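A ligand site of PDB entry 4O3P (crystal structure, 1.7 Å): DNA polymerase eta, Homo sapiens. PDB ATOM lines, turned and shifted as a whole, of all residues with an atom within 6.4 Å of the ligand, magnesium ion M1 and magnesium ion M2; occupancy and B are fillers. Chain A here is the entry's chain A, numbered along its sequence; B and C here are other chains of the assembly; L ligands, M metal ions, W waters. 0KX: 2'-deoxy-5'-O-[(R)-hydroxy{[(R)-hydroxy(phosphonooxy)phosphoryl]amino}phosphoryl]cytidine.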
ATOM      1  N   ASP A  16      24.098 -20.786 -17.108  1.00  0.00           N
ATOM      2  CA  ASP A  16      22.700 -20.914 -17.468  1.00  0.00           C
ATOM      3  C   ASP A  16      22.507 -22.080 -18.419  1.00  0.00           C
ATOM      4  O   ASP A  16      23.140 -22.143 -19.483  1.00  0.00           O
ATOM      5  CB  ASP A  16      22.181 -19.639 -18.114  1.00  0.00           C
ATOM      6  CG  ASP A  16      20.710 -19.720 -18.443  1.00  0.00           C
ATOM      7  OD1 ASP A  16      19.913 -19.174 -17.680  1.00  0.00           O
ATOM      8  OD2 ASP A  16      20.389 -20.365 -19.440  1.00  0.00           O
ATOM      9  N   MET A  17      21.580 -22.972 -18.097  1.00  0.00           N
ATOM     10  CA  MET A  17      21.417 -24.138 -18.959  1.00  0.00           C
ATOM     11  C   MET A  17      20.841 -23.792 -20.328  1.00  0.00           C
ATOM     12  O   MET A  17      19.993 -22.917 -20.458  1.00  0.00           O
ATOM     13  CB  MET A  17      20.506 -25.173 -18.295  1.00  0.00           C
ATOM     14  CG  MET A  17      20.927 -25.575 -16.878  1.00  0.00           C
ATOM     15  SD  MET A  17      22.597 -26.191 -16.748  1.00  0.00           S
ATOM     16  CE  MET A  17      22.532 -27.604 -17.784  1.00  0.00           C
ATOM     17  N   ASP A  18      21.307 -24.489 -21.363  1.00  0.00           N
ATOM     18  CA  ASP A  18      20.760 -24.243 -22.712  1.00  0.00           C
ATOM     19  C   ASP A  18      19.416 -24.927 -22.834  1.00  0.00           C
ATOM     20  O   ASP A  18      19.276 -26.070 -22.388  1.00  0.00           O
ATOM     21  CB  ASP A  18      21.705 -24.730 -23.806  1.00  0.00           C
ATOM     22  CG  ASP A  18      23.093 -24.022 -23.763  1.00  0.00           C
ATOM     23  OD1 ASP A  18      23.166 -22.869 -23.306  1.00  0.00           O
ATOM     24  OD2 ASP A  18      24.074 -24.624 -24.184  1.00  0.00           O
ATOM     25  N   CYS A  19      18.463 -24.223 -23.438  1.00  0.00           N
ATOM     26  CA  CYS A  19      17.063 -24.693 -23.652  1.00  0.00           C
ATOM     27  C   CYS A  19      16.662 -25.759 -22.628  1.00  0.00           C
ATOM     28  O   CYS A  19      16.413 -26.916 -22.944  1.00  0.00           O
ATOM     29  CB  CYS A  19      16.864 -25.181 -25.077  1.00  0.00           C
ATOM     30  SG  CYS A  19      18.008 -26.444 -25.719  1.00  0.00           S
ATOM     31  N   PHE A  20      16.657 -25.364 -21.376  1.00  0.00           N
ATOM     32  CA  PHE A  20      16.771 -26.344 -20.304  1.00  0.00           C
ATOM     33  C   PHE A  20      15.677 -27.429 -20.297  1.00  0.00           C
ATOM     34  O   PHE A  20      16.001 -28.612 -20.290  1.00  0.00           O
ATOM     35  CB  PHE A  20      16.787 -25.638 -18.956  1.00  0.00           C
ATOM     36  CG  PHE A  20      16.994 -26.570 -17.801  1.00  0.00           C
ATOM     37  CD1 PHE A  20      17.965 -27.574 -17.853  1.00  0.00           C
ATOM     38  CD2 PHE A  20      16.201 -26.440 -16.646  1.00  0.00           C
ATOM     39  CE1 PHE A  20      18.155 -28.432 -16.760  1.00  0.00           C
ATOM     40  CE2 PHE A  20      16.391 -27.312 -15.556  1.00  0.00           C
ATOM     41  CZ  PHE A  20      17.367 -28.293 -15.614  1.00  0.00           C
ATOM     42  N   PHE A  21      14.394 -27.037 -20.298  1.00  0.00           N
ATOM     43  CA  PHE A  21      13.364 -28.086 -20.181  1.00  0.00           C
ATOM     44  C   PHE A  21      13.445 -29.034 -21.393  1.00  0.00           C
ATOM     45  O   PHE A  21      13.156 -30.215 -21.300  1.00  0.00           O
ATOM     46  CB  PHE A  21      11.961 -27.511 -20.073  1.00  0.00           C
ATOM     47  CG  PHE A  21      11.638 -26.873 -18.740  1.00  0.00           C
ATOM     48  CD1 PHE A  21      12.623 -26.555 -17.818  1.00  0.00           C
ATOM     49  CD2 PHE A  21      10.313 -26.578 -18.425  1.00  0.00           C
ATOM     50  CE1 PHE A  21      12.263 -25.922 -16.573  1.00  0.00           C
ATOM     51  CE2 PHE A  21       9.960 -25.981 -17.212  1.00  0.00           C
ATOM     52  CZ  PHE A  21      10.949 -25.654 -16.300  1.00  0.00           C
ATOM     53  N   VAL A  22      13.782 -28.478 -22.552  1.00  0.00           N
ATOM     54  CA  VAL A  22      13.972 -29.308 -23.761  1.00  0.00           C
ATOM     55  C   VAL A  22      15.089 -30.344 -23.529  1.00  0.00           C
ATOM     56  O   VAL A  22      14.931 -31.537 -23.836  1.00  0.00           O
ATOM     57  CB  VAL A  22      14.291 -28.417 -25.000  1.00  0.00           C
ATOM     58  CG1 VAL A  22      14.795 -29.270 -26.180  1.00  0.00           C
ATOM     59  CG2 VAL A  22      13.006 -27.671 -25.443  1.00  0.00           C
ATOM     60  N   ILE A  51       6.834 -23.513 -23.676  1.00  0.00           N
ATOM     61  CA  ILE A  51       7.599 -22.867 -22.624  1.00  0.00           C
ATOM     62  C   ILE A  51       9.129 -23.054 -22.762  1.00  0.00           C
ATOM     63  O   ILE A  51       9.866 -22.382 -22.047  1.00  0.00           O
ATOM     64  CB  ILE A  51       7.160 -23.358 -21.262  1.00  0.00           C
ATOM     65  CG1 ILE A  51       7.329 -24.854 -21.135  1.00  0.00           C
ATOM     66  CG2 ILE A  51       5.683 -22.979 -21.025  1.00  0.00           C
ATOM     67  CD1 ILE A  51       7.105 -25.322 -19.674  1.00  0.00           C
ATOM     68  N   ALA A  52       9.594 -23.878 -23.722  1.00  0.00           N
ATOM     69  CA  ALA A  52      11.033 -24.046 -24.012  1.00  0.00           C
ATOM     70  C   ALA A  52      11.196 -24.564 -25.422  1.00  0.00           C
ATOM     71  O   ALA A  52      10.356 -25.327 -25.888  1.00  0.00           O
ATOM     72  CB  ALA A  52      11.706 -25.001 -23.006  1.00  0.00           C
ATOM     73  N   VAL A  53      12.265 -24.110 -26.096  1.00  0.00           N
ATOM     74  CA  VAL A  53      12.441 -24.354 -27.524  1.00  0.00           C
ATOM     75  C   VAL A  53      13.892 -24.721 -27.836  1.00  0.00           C
ATOM     76  O   VAL A  53      14.799 -23.986 -27.480  1.00  0.00           O
ATOM     77  CB  VAL A  53      12.072 -23.078 -28.326  1.00  0.00           C
ATOM     78  CG1 VAL A  53      12.071 -23.371 -29.848  1.00  0.00           C
ATOM     79  CG2 VAL A  53      10.741 -22.516 -27.878  1.00  0.00           C
ATOM     80  N   TYR A  55      17.376 -25.158 -29.984  1.00  0.00           N
ATOM     81  CA  TYR A  55      17.984 -24.202 -30.920  1.00  0.00           C
ATOM     82  C   TYR A  55      17.669 -24.529 -32.391  1.00  0.00           C
ATOM     83  O   TYR A  55      17.508 -23.597 -33.196  1.00  0.00           O
ATOM     84  CB  TYR A  55      19.501 -24.083 -30.668  1.00  0.00           C
ATOM     85  CG  TYR A  55      19.760 -23.228 -29.473  1.00  0.00           C
ATOM     86  CD1 TYR A  55      19.610 -23.732 -28.179  1.00  0.00           C
ATOM     87  CD2 TYR A  55      20.058 -21.870 -29.608  1.00  0.00           C
ATOM     88  CE1 TYR A  55      19.767 -22.902 -27.071  1.00  0.00           C
ATOM     89  CE2 TYR A  55      20.233 -21.044 -28.516  1.00  0.00           C
ATOM     90  CZ  TYR A  55      20.084 -21.549 -27.244  1.00  0.00           C
ATOM     91  OH  TYR A  55      20.276 -20.712 -26.142  1.00  0.00           O
ATOM     92  N   ARG A  58      14.359 -22.913 -32.882  1.00  0.00           N
ATOM     93  CA  ARG A  58      14.484 -21.446 -32.859  1.00  0.00           C
ATOM     94  C   ARG A  58      14.818 -20.918 -34.259  1.00  0.00           C
ATOM     95  O   ARG A  58      14.410 -19.811 -34.625  1.00  0.00           O
ATOM     96  CB  ARG A  58      15.556 -21.016 -31.878  1.00  0.00           C
ATOM     97  CG  ARG A  58      15.157 -21.217 -30.431  1.00  0.00           C
ATOM     98  CD  ARG A  58      16.217 -20.746 -29.437  1.00  0.00           C
ATOM     99  NE  ARG A  58      16.002 -21.413 -28.147  1.00  0.00           N
ATOM    100  CZ  ARG A  58      16.550 -21.043 -26.992  1.00  0.00           C
ATOM    101  NH1 ARG A  58      17.321 -19.956 -26.946  1.00  0.00           N
ATOM    102  NH2 ARG A  58      16.268 -21.743 -25.884  1.00  0.00           N
ATOM    103  N   ARG A  64       9.088 -19.087 -27.144  1.00  0.00           N
ATOM    104  CA  ARG A  64       8.306 -19.227 -25.933  1.00  0.00           C
ATOM    105  C   ARG A  64       7.003 -18.428 -26.049  1.00  0.00           C
ATOM    106  O   ARG A  64       6.988 -17.386 -26.705  1.00  0.00           O
ATOM    107  CB  ARG A  64       9.167 -18.749 -24.747  1.00  0.00           C
ATOM    108  CG  ARG A  64       8.463 -18.349 -23.460  1.00  0.00           C
ATOM    109  CD  ARG A  64       9.397 -17.462 -22.593  1.00  0.00           C
ATOM    110  NE  ARG A  64      10.679 -18.092 -22.269  1.00  0.00           N
ATOM    111  CZ  ARG A  64      11.876 -17.519 -22.413  1.00  0.00           C
ATOM    112  NH1 ARG A  64      11.992 -16.279 -22.892  1.00  0.00           N
ATOM    113  NH2 ARG A  64      12.982 -18.183 -22.093  1.00  0.00           N
ATOM    114  N   LEU A  92       5.740 -29.436 -12.334  1.00  0.00           N
ATOM    115  CA  LEU A  92       7.100 -29.209 -12.854  1.00  0.00           C
ATOM    116  C   LEU A  92       8.186 -30.005 -12.137  1.00  0.00           C
ATOM    117  O   LEU A  92       9.375 -29.696 -12.240  1.00  0.00           O
ATOM    118  CB  LEU A  92       7.424 -27.716 -12.769  1.00  0.00           C
ATOM    119  CG  LEU A  92       6.430 -26.872 -13.550  1.00  0.00           C
ATOM    120  CD1 LEU A  92       6.719 -25.414 -13.316  1.00  0.00           C
ATOM    121  CD2 LEU A  92       6.559 -27.227 -15.026  1.00  0.00           C
ATOM    122  N   SER A 116      17.566 -19.100 -10.673  1.00  0.00           N
ATOM    123  CA  SER A 116      16.355 -19.583 -11.322  1.00  0.00           C
ATOM    124  C   SER A 116      16.406 -21.103 -11.341  1.00  0.00           C
ATOM    125  O   SER A 116      17.372 -21.706 -10.885  1.00  0.00           O
ATOM    126  CB  SER A 116      16.234 -19.075 -12.757  1.00  0.00           C
ATOM    127  OG  SER A 116      17.108 -19.774 -13.654  1.00  0.00           O
ATOM    128  N   ILE A 117      15.395 -21.719 -11.927  1.00  0.00           N
ATOM    129  CA  ILE A 117      15.448 -23.170 -12.025  1.00  0.00           C
ATOM    130  C   ILE A 117      16.641 -23.623 -12.888  1.00  0.00           C
ATOM    131  O   ILE A 117      17.089 -24.775 -12.767  1.00  0.00           O
ATOM    132  CB  ILE A 117      14.120 -23.718 -12.617  1.00  0.00           C
ATOM    133  CG1 ILE A 117      13.976 -25.219 -12.347  1.00  0.00           C
ATOM    134  CG2 ILE A 117      14.091 -23.493 -14.138  1.00  0.00           C
ATOM    135  CD1 ILE A 117      12.578 -25.765 -12.697  1.00  0.00           C
ATOM    136  N   ASP A 118      17.190 -22.750 -13.745  1.00  0.00           N
ATOM    137  CA  ASP A 118      18.257 -23.260 -14.621  1.00  0.00           C
ATOM    138  C   ASP A 118      19.525 -22.413 -14.586  1.00  0.00           C
ATOM    139  O   ASP A 118      20.362 -22.542 -15.455  1.00  0.00           O
ATOM    140  CB  ASP A 118      17.759 -23.398 -16.081  1.00  0.00           C
ATOM    141  CG  ASP A 118      17.978 -22.140 -16.924  1.00  0.00           C
ATOM    142  OD1 ASP A 118      17.757 -21.014 -16.418  1.00  0.00           O
ATOM    143  OD2 ASP A 118      18.433 -22.338 -18.062  1.00  0.00           O
ATOM    144  N   GLU A 119      19.694 -21.567 -13.573  1.00  0.00           N
ATOM    145  CA  GLU A 119      20.962 -20.821 -13.542  1.00  0.00           C
ATOM    146  C   GLU A 119      21.386 -20.463 -12.134  1.00  0.00           C
ATOM    147  O   GLU A 119      20.559 -20.374 -11.225  1.00  0.00           O
ATOM    148  CB  GLU A 119      20.871 -19.560 -14.399  1.00  0.00           C
ATOM    149  CG  GLU A 119      19.996 -18.489 -13.801  1.00  0.00           C
ATOM    150  CD  GLU A 119      19.343 -17.670 -14.879  1.00  0.00           C
ATOM    151  OE1 GLU A 119      18.375 -18.160 -15.487  1.00  0.00           O
ATOM    152  OE2 GLU A 119      19.837 -16.560 -15.171  1.00  0.00           O
ATOM    153  N   SER A 216      25.715 -22.668 -21.023  1.00  0.00           N
ATOM    154  CA  SER A 216      26.606 -21.565 -21.335  1.00  0.00           C
ATOM    155  C   SER A 216      26.952 -20.841 -20.037  1.00  0.00           C
ATOM    156  O   SER A 216      26.351 -21.112 -18.981  1.00  0.00           O
ATOM    157  CB  SER A 216      25.941 -20.633 -22.339  1.00  0.00           C
ATOM    158  OG  SER A 216      25.696 -21.373 -23.529  1.00  0.00           O
ATOM    159  N   LYS A 227      25.896 -12.179 -16.257  1.00  0.00           N
ATOM    160  CA  LYS A 227      24.629 -12.575 -16.859  1.00  0.00           C
ATOM    161  C   LYS A 227      24.577 -12.124 -18.316  1.00  0.00           C
ATOM    162  O   LYS A 227      24.178 -12.888 -19.196  1.00  0.00           O
ATOM    163  CB  LYS A 227      23.430 -11.987 -16.098  1.00  0.00           C
ATOM    164  CG  LYS A 227      22.072 -12.290 -16.737  1.00  0.00           C
ATOM    165  CD  LYS A 227      21.773 -13.808 -16.813  1.00  0.00           C
ATOM    166  CE  LYS A 227      20.313 -14.003 -17.334  1.00  0.00           C
ATOM    167  NZ  LYS A 227      19.810 -15.401 -17.657  1.00  0.00           N
ATOM    168  N   LYS A 234      25.624 -18.059 -26.421  1.00  0.00           N
ATOM    169  CA  LYS A 234      24.762 -19.252 -26.342  1.00  0.00           C
ATOM    170  C   LYS A 234      24.507 -19.783 -27.731  1.00  0.00           C
ATOM    171  O   LYS A 234      24.307 -18.971 -28.664  1.00  0.00           O
ATOM    172  CB  LYS A 234      23.411 -18.912 -25.700  1.00  0.00           C
ATOM    173  CG  LYS A 234      23.359 -19.068 -24.236  1.00  0.00           C
ATOM    174  CD  LYS A 234      21.942 -19.007 -23.692  1.00  0.00           C
ATOM    175  CE  LYS A 234      21.942 -19.331 -22.178  1.00  0.00           C
ATOM    176  NZ  LYS A 234      21.836 -20.843 -21.930  1.00  0.00           N
ATOM    177  N   PRO A 235      24.402 -21.115 -27.896  1.00  0.00           N
ATOM    178  CA  PRO A 235      24.493 -22.130 -26.827  1.00  0.00           C
ATOM    179  C   PRO A 235      25.874 -22.779 -26.714  1.00  0.00           C
ATOM    180  O   PRO A 235      26.721 -22.703 -27.618  1.00  0.00           O
ATOM    181  CB  PRO A 235      23.453 -23.175 -27.260  1.00  0.00           C
ATOM    182  CG  PRO A 235      23.616 -23.191 -28.786  1.00  0.00           C
ATOM    183  CD  PRO A 235      23.958 -21.723 -29.170  1.00  0.00           C
ATOM    184  P    DT B   8      15.217 -13.107 -17.172  1.00  0.00           P
ATOM    185  OP1  DT B   8      16.626 -13.002 -17.619  1.00  0.00           O
ATOM    186  OP2  DT B   8      14.056 -12.782 -18.064  1.00  0.00           O
ATOM    187  O5'  DT B   8      14.908 -14.563 -16.602  1.00  0.00           O
ATOM    188  C5'  DT B   8      15.714 -15.182 -15.629  1.00  0.00           C
ATOM    189  C4'  DT B   8      15.198 -16.587 -15.439  1.00  0.00           C
ATOM    190  O4'  DT B   8      13.807 -16.540 -15.022  1.00  0.00           O
ATOM    191  C3'  DT B   8      15.249 -17.434 -16.701  1.00  0.00           C
ATOM    192  O3'  DT B   8      15.767 -18.741 -16.404  1.00  0.00           O
ATOM    193  C2'  DT B   8      13.783 -17.478 -17.182  1.00  0.00           C
ATOM    194  C1'  DT B   8      13.013 -17.341 -15.882  1.00  0.00           C
ATOM    195  N1   DT B   8      11.690 -16.695 -16.021  1.00  0.00           N
ATOM    196  C2   DT B   8      10.567 -17.369 -15.571  1.00  0.00           C
ATOM    197  O2   DT B   8      10.601 -18.477 -15.097  1.00  0.00           O
ATOM    198  N3   DT B   8       9.394 -16.676 -15.695  1.00  0.00           N
ATOM    199  C4   DT B   8       9.241 -15.404 -16.224  1.00  0.00           C
ATOM    200  O4   DT B   8       8.141 -14.858 -16.298  1.00  0.00           O
ATOM    201  C5   DT B   8      10.453 -14.764 -16.674  1.00  0.00           C
ATOM    202  C7   DT B   8      10.395 -13.375 -17.251  1.00  0.00           C
ATOM    203  C6   DT B   8      11.597 -15.427 -16.546  1.00  0.00           C
ATOM    204  P    DT C   3      -3.312 -14.927 -24.637  1.00  0.00           P
ATOM    205  OP1  DT C   3      -4.031 -13.685 -24.984  1.00  0.00           O
ATOM    206  OP2  DT C   3      -2.329 -15.510 -25.585  1.00  0.00           O
ATOM    207  O5'  DT C   3      -2.592 -14.717 -23.217  1.00  0.00           O
ATOM    208  C5'  DT C   3      -1.243 -15.159 -23.021  1.00  0.00           C
ATOM    209  C4'  DT C   3      -1.202 -16.650 -22.711  1.00  0.00           C
ATOM    210  O4'  DT C   3       0.123 -17.174 -23.009  1.00  0.00           O
ATOM    211  C3'  DT C   3      -1.512 -17.015 -21.265  1.00  0.00           C
ATOM    212  O3'  DT C   3      -2.581 -17.995 -21.216  1.00  0.00           O
ATOM    213  C2'  DT C   3      -0.170 -17.531 -20.703  1.00  0.00           C
ATOM    214  C1'  DT C   3       0.583 -17.981 -21.941  1.00  0.00           C
ATOM    215  N1   DT C   3       2.110 -17.803 -21.846  1.00  0.00           N
ATOM    216  C2   DT C   3       2.949 -18.915 -21.934  1.00  0.00           C
ATOM    217  O2   DT C   3       2.545 -20.067 -22.060  1.00  0.00           O
ATOM    218  N3   DT C   3       4.289 -18.630 -21.848  1.00  0.00           N
ATOM    219  C4   DT C   3       4.870 -17.374 -21.710  1.00  0.00           C
ATOM    220  O4   DT C   3       6.088 -17.223 -21.649  1.00  0.00           O
ATOM    221  C5   DT C   3       3.939 -16.253 -21.639  1.00  0.00           C
ATOM    222  C7   DT C   3       4.464 -14.853 -21.481  1.00  0.00           C
ATOM    223  C6   DT C   3       2.623 -16.519 -21.715  1.00  0.00           C
ATOM    224  P   8OG C   4      -3.221 -18.466 -19.807  1.00  0.00           P
ATOM    225  OP1 8OG C   4      -3.497 -17.276 -18.920  1.00  0.00           O
ATOM    226  OP2 8OG C   4      -4.365 -19.402 -20.132  1.00  0.00           O
ATOM    227  O5' 8OG C   4      -2.042 -19.315 -19.129  1.00  0.00           O
ATOM    228  C5' 8OG C   4      -1.626 -20.585 -19.594  1.00  0.00           C
ATOM    229  C4' 8OG C   4      -0.623 -21.090 -18.558  1.00  0.00           C
ATOM    230  O4' 8OG C   4       0.679 -20.510 -18.749  1.00  0.00           O
ATOM    231  C3' 8OG C   4      -1.032 -20.821 -17.126  1.00  0.00           C
ATOM    232  O3' 8OG C   4      -0.858 -22.099 -16.487  1.00  0.00           O
ATOM    233  C2' 8OG C   4      -0.013 -19.825 -16.604  1.00  0.00           C
ATOM    234  C1' 8OG C   4       1.203 -20.172 -17.457  1.00  0.00           C
ATOM    235  N9  8OG C   4       2.147 -19.065 -17.707  1.00  0.00           N
ATOM    236  C8  8OG C   4       2.035 -17.744 -17.904  1.00  0.00           C
ATOM    237  N7  8OG C   4       3.186 -17.097 -18.135  1.00  0.00           N
ATOM    238  C5  8OG C   4       4.114 -18.084 -18.097  1.00  0.00           C
ATOM    239  C6  8OG C   4       5.567 -18.164 -18.272  1.00  0.00           C
ATOM    240  O6  8OG C   4       6.219 -17.129 -18.497  1.00  0.00           O
ATOM    241  N1  8OG C   4       6.138 -19.385 -18.159  1.00  0.00           N
ATOM    242  C2  8OG C   4       5.445 -20.506 -17.903  1.00  0.00           C
ATOM    243  N2  8OG C   4       6.085 -21.683 -17.775  1.00  0.00           N
ATOM    244  N3  8OG C   4       4.095 -20.503 -17.731  1.00  0.00           N
ATOM    245  C4  8OG C   4       3.431 -19.345 -17.837  1.00  0.00           C
ATOM    246  O8  8OG C   4       0.921 -17.111 -17.857  1.00  0.00           O
ATOM    247  P    DA C   5      -1.092 -22.326 -14.909  1.00  0.00           P
ATOM    248  OP1  DA C   5      -1.796 -23.596 -14.816  1.00  0.00           O
ATOM    249  OP2  DA C   5      -1.669 -21.117 -14.279  1.00  0.00           O
ATOM    250  O5'  DA C   5       0.390 -22.482 -14.323  1.00  0.00           O
ATOM    251  C5'  DA C   5       1.223 -23.579 -14.747  1.00  0.00           C
ATOM    252  C4'  DA C   5       2.544 -23.554 -14.009  1.00  0.00           C
ATOM    253  O4'  DA C   5       3.362 -22.465 -14.519  1.00  0.00           O
ATOM    254  C3'  DA C   5       2.417 -23.331 -12.503  1.00  0.00           C
ATOM    255  O3'  DA C   5       3.444 -24.080 -11.844  1.00  0.00           O
ATOM    256  C2'  DA C   5       2.678 -21.829 -12.378  1.00  0.00           C
ATOM    257  C1'  DA C   5       3.759 -21.652 -13.445  1.00  0.00           C
ATOM    258  N9   DA C   5       3.910 -20.290 -13.924  1.00  0.00           N
ATOM    259  C8   DA C   5       2.925 -19.361 -14.100  1.00  0.00           C
ATOM    260  N7   DA C   5       3.361 -18.208 -14.558  1.00  0.00           N
ATOM    261  C5   DA C   5       4.722 -18.393 -14.672  1.00  0.00           C
ATOM    262  C6   DA C   5       5.758 -17.528 -15.083  1.00  0.00           C
ATOM    263  N6   DA C   5       5.542 -16.260 -15.490  1.00  0.00           N
ATOM    264  N1   DA C   5       7.006 -18.011 -15.084  1.00  0.00           N
ATOM    265  C2   DA C   5       7.210 -19.281 -14.696  1.00  0.00           C
ATOM    266  N3   DA C   5       6.315 -20.177 -14.277  1.00  0.00           N
ATOM    267  C4   DA C   5       5.078 -19.661 -14.291  1.00  0.00           C
HETATM  268  PG  0KX L   1      18.370 -20.644 -23.159  1.00  0.00           P
HETATM  269  O1G 0KX L   1      18.759 -20.337 -21.744  1.00  0.00           O
HETATM  270  O2G 0KX L   1      18.039 -19.408 -24.012  1.00  0.00           O
HETATM  271  O3G 0KX L   1      19.391 -21.492 -23.833  1.00  0.00           O
HETATM  272  PB  0KX L   1      16.198 -21.790 -21.811  1.00  0.00           P
HETATM  273  O1B 0KX L   1      17.076 -22.409 -20.760  1.00  0.00           O
HETATM  274  O2B 0KX L   1      15.040 -22.669 -22.245  1.00  0.00           O
HETATM  275  O3B 0KX L   1      16.993 -21.463 -23.105  1.00  0.00           O
HETATM  276  PA  0KX L   1      15.785 -19.752 -19.680  1.00  0.00           P
HETATM  277  O1A 0KX L   1      15.297 -18.301 -19.768  1.00  0.00           O
HETATM  278  O2A 0KX L   1      17.142 -19.953 -19.127  1.00  0.00           O
HETATM  279  N3A 0KX L   1      15.663 -20.309 -21.260  1.00  0.00           N
HETATM  280  O5' 0KX L   1      14.724 -20.557 -18.822  1.00  0.00           O
HETATM  281  C5' 0KX L   1      15.019 -21.847 -18.281  1.00  0.00           C
HETATM  282  C4' 0KX L   1      13.837 -22.682 -18.262  1.00  0.00           C
HETATM  283  O4' 0KX L   1      12.747 -22.033 -17.386  1.00  0.00           O
HETATM  284  C3' 0KX L   1      13.132 -22.849 -19.622  1.00  0.00           C
HETATM  285  O3' 0KX L   1      13.717 -23.994 -20.302  1.00  0.00           O
HETATM  286  C2' 0KX L   1      11.827 -23.093 -19.312  1.00  0.00           C
HETATM  287  C1' 0KX L   1      11.559 -22.251 -17.984  1.00  0.00           C
HETATM  288  N1  0KX L   1      10.962 -20.991 -18.283  1.00  0.00           N
HETATM  289  C2  0KX L   1       9.522 -20.867 -18.110  1.00  0.00           C
HETATM  290  N3  0KX L   1       8.909 -19.605 -18.383  1.00  0.00           N
HETATM  291  C4  0KX L   1       9.648 -18.490 -18.834  1.00  0.00           C
HETATM  292  C5  0KX L   1      11.093 -18.607 -19.038  1.00  0.00           C
HETATM  293  C6  0KX L   1      11.727 -19.890 -18.743  1.00  0.00           C
HETATM  294  O2  0KX L   1       8.871 -21.843 -17.711  1.00  0.00           O
HETATM  295  N4  0KX L   1       9.004 -17.254 -19.116  1.00  0.00           N
HETATM  296 MG    MG M   1      18.657 -21.343 -19.920  1.00  0.00          MG
HETATM  297 MG    MG M   2      17.902 -19.133 -17.263  1.00  0.00          MG
HETATM  298  O   HOH W   1      14.058 -20.286 -15.577  1.00  0.00           O
HETATM  299  O   HOH W   2      15.499 -15.642 -20.407  1.00  0.00           O
HETATM  300  O   HOH W   3      17.856 -17.333 -18.483  1.00  0.00           O
HETATM  301  O   HOH W   4      13.750 -22.216 -24.539  1.00  0.00           O
HETATM  302  O   HOH W   5      10.752 -15.309 -20.309  1.00  0.00           O
HETATM  303  O   HOH W   6      10.937 -21.219 -14.641  1.00  0.00           O
HETATM  304  O   HOH W   7      15.518 -18.438 -23.714  1.00  0.00           O
HETATM  305  O   HOH W   8      19.106 -17.679 -20.910  1.00  0.00           O
HETATM  306  O   HOH W   9       8.050 -23.690 -16.032  1.00  0.00           O
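A nitrogen (N4) of the ligand sits close to N3 of DT 8 of chain B (3.5 Å). The side-chain hydroxyl (OH) of Tyr 55 is in hydrogen-bond range of an oxygen (O3G) of the ligand, 2.6 Å away. O6 of 8OG 4 of chain C sits at hydrogen-bond distance from N4 of the ligand, 2.9 Å away. O2G of the ligand lies within salt-bridge range of NH1 of Arg 58 (3.1 Å). N of Cys 19 sits at hydrogen-bond distance from O3G of the ligand, at 2.9 Å. O2B of the ligand lies within hydrogen-bond range of N of Phe 20, at 3.3 Å. The backbone NH (N) of Phe 21 sits at hydrogen-bond distance from an oxygen (O3') of the ligand, 3.1 Å away. The side-chain amino group of Lys 234 is in salt-bridge range of an oxygen (O3G) of the ligand, 3.2 Å away. The guanidinium group of Arg 64 is in salt-bridge range of an oxygen (O1A) of the ligand, 3.3 Å away.
The backbone NH (N) of Asp 16 sits at hydrogen-bond distance from the backbone carbonyl oxygen (O) of Ser 216. N of Asp 118 is in hydrogen-bond range of OG of Ser 116, 3.0 Å away. The side-chain hydroxyl of Ser 116 is in hydrogen-bond range of the backbone NH of Glu 119 (3.1 Å). The side-chain amino group of Lys 227 is in salt-bridge range of the side-chain carboxylate of Glu 119, 2.7 Å away. The backbone carbonyl oxygen of Met 17 sits close to the side-chain amino group of Lys 234 (3.1 Å). The side-chain hydroxyl (OG) of Ser 116 lies close to O3' of DT 8 of chain B, at 3.2 Å. The side-chain hydroxyl of Tyr 55 is in hydrogen-bond range of the guanidinium group of Arg 58 (3.2 Å). The side-chain amino group of Lys 234 lies within salt-bridge range of the side-chain carboxylate of Asp 18 (2.8 Å).
Asp 18 touches the ligand (CA to O3G, 3.3 Å). O of Ile 51 touches C2' of the ligand (3.4 Å). Ala 52 touches the ligand. CG2 of Ile 117 touches O4' of the ligand (3.8 Å). DT 3 of chain C touches the ligand. Of the 26 residues printed, 17 come within 4 Å of the ligand. The nearest printed residue that does not touch the ligand is DA 5 of chain C (4.1 Å).
Residues that only touch magnesium ion M1: Lys 234 (3.8 Å). Within 4 Å of magnesium ion M1: Asp 16, Met 17, Asp 118 and Lys 234.
Ser 116 touches magnesium ion M2. Of the 26 residues printed, 5 come within 4 Å of magnesium ion M2. Along chain A the residues within 4 Å of magnesium ion M2 span positions 16 to 119. The nearest printed residue that does not touch magnesium ion M2 is Lys 227 (4.2 Å).
Magnesium ion M1 is bound by OD2 of Asp 16, O1B of the ligand, O1G of the ligand, OD2 of Asp 118, O of Met 17 and O2A of the ligand. Magnesium ion M1 has six donor atoms within binding distance.
Magnesium ion M2 is bound by OD1 of Asp 16 (2.1 Å), OD1 of Asp 118 (2.1 Å), OE1 of Glu 119 (2.1 Å), O2A of the ligand (2.2 Å), water W3 (2.2 Å) and O3' of DT 8 of chain B (2.3 Å).
Water W3 lies within hydrogen-bond range of NZ of Lys 227 (2.9 Å) and O1A of the ligand (3.0 Å). Water W9 lies within hydrogen-bond range of O2 of the ligand (2.6 Å) and N2 of 8OG 4 of chain C (3.3 Å). Water W4 lies within hydrogen-bond range of O2B of the ligand (2.7 Å), N of Val 53 (2.9 Å) and NH2 of Arg 58 (2.9 Å). Water W7 bridges an oxygen (O2G) of the ligand and the guanidinium group of Arg 64. Water W5 lies within hydrogen-bond range of a nitrogen (N4) of the ligand and the guanidinium group of Arg 64. Water W6 lies within hydrogen-bond range of O2 of DT 8 of chain B and an oxygen (O4') of the ligand.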
